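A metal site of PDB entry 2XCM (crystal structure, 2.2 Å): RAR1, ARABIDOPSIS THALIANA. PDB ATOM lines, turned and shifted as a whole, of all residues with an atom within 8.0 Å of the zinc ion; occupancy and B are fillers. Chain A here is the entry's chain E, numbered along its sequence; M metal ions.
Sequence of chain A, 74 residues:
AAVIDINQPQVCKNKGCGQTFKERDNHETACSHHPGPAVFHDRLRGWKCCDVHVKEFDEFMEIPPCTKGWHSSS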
ATOM      1  N   LYS A  15     -15.306   2.936  -1.261  1.00  0.00           N
ATOM      2  CA  LYS A  15     -16.649   3.398  -1.611  1.00  0.00           C
ATOM      3  C   LYS A  15     -17.414   3.941  -0.401  1.00  0.00           C
ATOM      4  O   LYS A  15     -17.601   3.234   0.604  1.00  0.00           O
ATOM      5  CB  LYS A  15     -17.447   2.266  -2.302  1.00  0.00           C
ATOM      6  CG  LYS A  15     -16.862   1.778  -3.662  1.00  0.00           C
ATOM      7  CD  LYS A  15     -17.588   0.511  -4.212  1.00  0.00           C
ATOM      8  CE  LYS A  15     -17.168   0.141  -5.656  1.00  0.00           C
ATOM      9  NZ  LYS A  15     -18.129  -0.790  -6.430  1.00  0.00           N
ATOM     10  N   HIS A  33     -17.073   2.353   5.009  1.00  0.00           N
ATOM     11  CA  HIS A  33     -17.189   2.213   3.563  1.00  0.00           C
ATOM     12  C   HIS A  33     -17.924   0.917   3.232  1.00  0.00           C
ATOM     13  O   HIS A  33     -18.060   0.038   4.093  1.00  0.00           O
ATOM     14  CB  HIS A  33     -15.789   2.178   2.958  1.00  0.00           C
ATOM     15  CG  HIS A  33     -14.973   1.000   3.417  1.00  0.00           C
ATOM     16  ND1 HIS A  33     -14.632  -0.039   2.585  1.00  0.00           N
ATOM     17  CD2 HIS A  33     -14.474   0.693   4.634  1.00  0.00           C
ATOM     18  CE1 HIS A  33     -13.940  -0.939   3.272  1.00  0.00           C
ATOM     19  NE2 HIS A  33     -13.831  -0.509   4.520  1.00  0.00           N
ATOM     20  N   HIS A  34     -18.397   0.809   1.994  1.00  0.00           N
ATOM     21  CA  HIS A  34     -18.879  -0.471   1.422  1.00  0.00           C
ATOM     22  C   HIS A  34     -17.691  -1.140   0.729  1.00  0.00           C
ATOM     23  O   HIS A  34     -17.168  -0.584  -0.234  1.00  0.00           O
ATOM     24  CB  HIS A  34     -19.955  -0.252   0.325  1.00  0.00           C
ATOM     25  CG  HIS A  34     -21.299   0.174   0.826  1.00  0.00           C
ATOM     26  ND1 HIS A  34     -22.178  -0.679   1.458  1.00  0.00           N
ATOM     27  CD2 HIS A  34     -21.937   1.372   0.736  1.00  0.00           C
ATOM     28  CE1 HIS A  34     -23.287  -0.031   1.765  1.00  0.00           C
ATOM     29  NE2 HIS A  34     -23.177   1.221   1.338  1.00  0.00           N
ATOM     30  N   PRO A  35     -17.273  -2.332   1.199  1.00  0.00           N
ATOM     31  CA  PRO A  35     -16.216  -3.024   0.441  1.00  0.00           C
ATOM     32  C   PRO A  35     -16.660  -3.363  -0.977  1.00  0.00           C
ATOM     33  O   PRO A  35     -15.810  -3.493  -1.861  1.00  0.00           O
ATOM     34  CB  PRO A  35     -15.969  -4.306   1.249  1.00  0.00           C
ATOM     35  CG  PRO A  35     -16.416  -3.983   2.637  1.00  0.00           C
ATOM     36  CD  PRO A  35     -17.579  -3.014   2.470  1.00  0.00           C
ATOM     37  N   GLY A  36     -17.974  -3.497  -1.195  1.00  0.00           N
ATOM     38  CA  GLY A  36     -18.513  -3.735  -2.525  1.00  0.00           C
ATOM     39  C   GLY A  36     -18.381  -5.191  -2.915  1.00  0.00           C
ATOM     40  O   GLY A  36     -18.030  -6.017  -2.068  1.00  0.00           O
ATOM     41  N   PRO A  37     -18.667  -5.539  -4.177  1.00  0.00           N
ATOM     42  CA  PRO A  37     -19.101  -4.663  -5.271  1.00  0.00           C
ATOM     43  C   PRO A  37     -20.588  -4.296  -5.178  1.00  0.00           C
ATOM     44  O   PRO A  37     -21.352  -4.943  -4.476  1.00  0.00           O
ATOM     45  CB  PRO A  37     -18.920  -5.544  -6.529  1.00  0.00           C
ATOM     46  CG  PRO A  37     -18.754  -6.964  -6.028  1.00  0.00           C
ATOM     47  CD  PRO A  37     -18.724  -6.972  -4.535  1.00  0.00           C
ATOM     48  N   GLY A  46     -28.128  -2.880  -5.247  1.00  0.00           N
ATOM     49  CA  GLY A  46     -27.628  -3.136  -3.904  1.00  0.00           C
ATOM     50  C   GLY A  46     -26.138  -3.322  -3.793  1.00  0.00           C
ATOM     51  O   GLY A  46     -25.395  -3.081  -4.733  1.00  0.00           O
ATOM     52  N   TRP A  47     -25.721  -3.801  -2.622  1.00  0.00           N
ATOM     53  CA  TRP A  47     -24.320  -3.943  -2.267  1.00  0.00           C
ATOM     54  C   TRP A  47     -24.108  -5.373  -1.776  1.00  0.00           C
ATOM     55  O   TRP A  47     -24.819  -5.846  -0.894  1.00  0.00           O
ATOM     56  CB  TRP A  47     -23.949  -2.948  -1.134  1.00  0.00           C
ATOM     57  CG  TRP A  47     -23.873  -1.543  -1.592  1.00  0.00           C
ATOM     58  CD1 TRP A  47     -24.792  -0.562  -1.391  1.00  0.00           C
ATOM     59  CD2 TRP A  47     -22.812  -0.934  -2.344  1.00  0.00           C
ATOM     60  NE1 TRP A  47     -24.372   0.606  -1.954  1.00  0.00           N
ATOM     61  CE2 TRP A  47     -23.157   0.401  -2.551  1.00  0.00           C
ATOM     62  CE3 TRP A  47     -21.597  -1.414  -2.851  1.00  0.00           C
ATOM     63  CZ2 TRP A  47     -22.335   1.288  -3.264  1.00  0.00           C
ATOM     64  CZ3 TRP A  47     -20.787  -0.551  -3.556  1.00  0.00           C
ATOM     65  CH2 TRP A  47     -21.165   0.796  -3.750  1.00  0.00           C
ATOM     66  N   LYS A  48     -23.136  -6.058  -2.369  1.00  0.00           N
ATOM     67  CA  LYS A  48     -22.874  -7.447  -2.002  1.00  0.00           C
ATOM     68  C   LYS A  48     -22.234  -7.583  -0.610  1.00  0.00           C
ATOM     69  O   LYS A  48     -22.437  -8.584   0.058  1.00  0.00           O
ATOM     70  CB  LYS A  48     -21.996  -8.119  -3.063  1.00  0.00           C
ATOM     71  CG  LYS A  48     -21.809  -9.619  -2.844  1.00  0.00           C
ATOM     72  CD  LYS A  48     -21.288 -10.288  -4.124  1.00  0.00           C
ATOM     73  CE  LYS A  48     -19.867 -10.776  -3.959  1.00  0.00           C
ATOM     74  NZ  LYS A  48     -19.802 -11.921  -3.009  1.00  0.00           N
ATOM     75  N   CYS A  49     -21.494  -6.560  -0.180  1.00  0.00           N
ATOM     76  CA  CYS A  49     -20.817  -6.599   1.113  1.00  0.00           C
ATOM     77  C   CYS A  49     -21.799  -6.748   2.273  1.00  0.00           C
ATOM     78  O   CYS A  49     -21.628  -7.628   3.115  1.00  0.00           O
ATOM     79  CB  CYS A  49     -19.944  -5.345   1.301  1.00  0.00           C
ATOM     80  SG  CYS A  49     -20.632  -3.811   0.596  1.00  0.00           S
ATOM     81  N   CYS A  50     -22.828  -5.915   2.314  1.00  0.00           N
ATOM     82  CA  CYS A  50     -23.834  -6.001   3.381  1.00  0.00           C
ATOM     83  C   CYS A  50     -25.114  -6.732   2.954  1.00  0.00           C
ATOM     84  O   CYS A  50     -26.029  -6.928   3.750  1.00  0.00           O
ATOM     85  CB  CYS A  50     -24.167  -4.594   3.895  1.00  0.00           C
ATOM     86  SG  CYS A  50     -24.213  -3.312   2.597  1.00  0.00           S
ATOM     87  N   ASP A  51     -25.175  -7.119   1.685  1.00  0.00           N
ATOM     88  CA  ASP A  51     -26.307  -7.867   1.158  1.00  0.00           C
ATOM     89  C   ASP A  51     -27.615  -7.099   1.332  1.00  0.00           C
ATOM     90  O   ASP A  51     -28.613  -7.681   1.712  1.00  0.00           O
ATOM     91  CB  ASP A  51     -26.435  -9.232   1.857  1.00  0.00           C
ATOM     92  CG  ASP A  51     -27.299 -10.214   1.070  1.00  0.00           C
ATOM     93  OD1 ASP A  51     -27.078 -10.371  -0.154  1.00  0.00           O
ATOM     94  OD2 ASP A  51     -28.203 -10.841   1.679  1.00  0.00           O
ATOM     95  N   VAL A  52     -27.602  -5.795   1.092  1.00  0.00           N
ATOM     96  CA  VAL A  52     -28.850  -5.044   1.081  1.00  0.00           C
ATOM     97  C   VAL A  52     -29.173  -4.654  -0.365  1.00  0.00           C
ATOM     98  O   VAL A  52     -28.320  -4.115  -1.063  1.00  0.00           O
ATOM     99  CB  VAL A  52     -28.831  -3.799   2.001  1.00  0.00           C
ATOM    100  CG1 VAL A  52     -28.328  -4.149   3.413  1.00  0.00           C
ATOM    101  CG2 VAL A  52     -27.970  -2.728   1.402  1.00  0.00           C
ATOM    102  N   ILE A  63     -27.904   3.725   0.642  1.00  0.00           N
ATOM    103  CA  ILE A  63     -27.578   2.642   1.572  1.00  0.00           C
ATOM    104  C   ILE A  63     -26.252   2.978   2.239  1.00  0.00           C
ATOM    105  O   ILE A  63     -25.248   3.139   1.564  1.00  0.00           O
ATOM    106  CB  ILE A  63     -27.515   1.274   0.901  1.00  0.00           C
ATOM    107  CG1 ILE A  63     -28.844   0.958   0.238  1.00  0.00           C
ATOM    108  CG2 ILE A  63     -27.174   0.215   1.947  1.00  0.00           C
ATOM    109  CD1 ILE A  63     -28.723  -0.065  -0.867  1.00  0.00           C
ATOM    110  N   PRO A  64     -26.261   3.115   3.566  1.00  0.00           N
ATOM    111  CA  PRO A  64     -25.108   3.565   4.341  1.00  0.00           C
ATOM    112  C   PRO A  64     -23.976   2.547   4.342  1.00  0.00           C
ATOM    113  O   PRO A  64     -24.218   1.337   4.331  1.00  0.00           O
ATOM    114  CB  PRO A  64     -25.659   3.716   5.776  1.00  0.00           C
ATOM    115  CG  PRO A  64     -27.144   3.723   5.630  1.00  0.00           C
ATOM    116  CD  PRO A  64     -27.439   2.869   4.419  1.00  0.00           C
ATOM    117  N   PRO A  65     -22.734   3.037   4.338  1.00  0.00           N
ATOM    118  CA  PRO A  65     -21.500   2.253   4.470  1.00  0.00           C
ATOM    119  C   PRO A  65     -21.692   1.221   5.555  1.00  0.00           C
ATOM    120  O   PRO A  65     -22.303   1.514   6.589  1.00  0.00           O
ATOM    121  CB  PRO A  65     -20.473   3.298   4.898  1.00  0.00           C
ATOM    122  CG  PRO A  65     -20.931   4.535   4.185  1.00  0.00           C
ATOM    123  CD  PRO A  65     -22.448   4.475   4.211  1.00  0.00           C
ATOM    124  N   CYS A  66     -21.204   0.009   5.333  1.00  0.00           N
ATOM    125  CA  CYS A  66     -21.553  -1.097   6.208  1.00  0.00           C
ATOM    126  C   CYS A  66     -20.354  -1.602   7.003  1.00  0.00           C
ATOM    127  O   CYS A  66     -20.520  -2.392   7.914  1.00  0.00           O
ATOM    128  CB  CYS A  66     -22.075  -2.265   5.370  1.00  0.00           C
ATOM    129  SG  CYS A  66     -20.790  -2.918   4.279  1.00  0.00           S
ATOM    130  N   THR A  67     -19.146  -1.168   6.634  1.00  0.00           N
ATOM    131  CA  THR A  67     -17.931  -1.778   7.163  1.00  0.00           C
ATOM    132  C   THR A  67     -16.930  -0.754   7.685  1.00  0.00           C
ATOM    133  O   THR A  67     -16.757   0.312   7.091  1.00  0.00           O
ATOM    134  CB  THR A  67     -17.231  -2.621   6.067  1.00  0.00           C
ATOM    135  OG1 THR A  67     -18.113  -3.646   5.618  1.00  0.00           O
ATOM    136  CG2 THR A  67     -15.956  -3.264   6.611  1.00  0.00           C
HETATM  137 ZN    ZN M   1     -21.942  -2.724   2.185  1.00  0.00          ZN
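The zinc ion is bound by a ring nitrogen (ND1) of His 34 (2.2 Å), the side-chain sulfur of Cys 49 (2.3 Å), the side-chain sulfur of Cys 50 (2.4 Å) and the side-chain sulfur of Cys 66 (2.4 Å).
The zinc ion has four donor atoms within binding distance.
Residues that only touch the zinc ion: Trp 47.
Of the 18 residues printed, 5 come within 4 Å of the zinc ion.
N of Cys 66 sits at hydrogen-bond distance from O of His 33, at 3.4 Å.
The side-chain hydroxyl (OG1) of Thr 67 lies close to the side-chain sulfur (SG) of Cys 66.
The backbone NH (N) of His 34 is in hydrogen-bond range of the backbone carbonyl oxygen (O) of Lys 15 (2.9 Å).
NE2 of His 34 sits close to O of Pro 64 (3.2 Å).
A ring nitrogen (NE2) of His 34 is in hydrogen-bond range of the backbone carbonyl oxygen (O) of Ile 63 (2.8 Å).
O of Val 52 sits at hydrogen-bond distance from N of Trp 47, at 3.0 Å.
N of Gly 36 lies close to SG of Cys 49.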
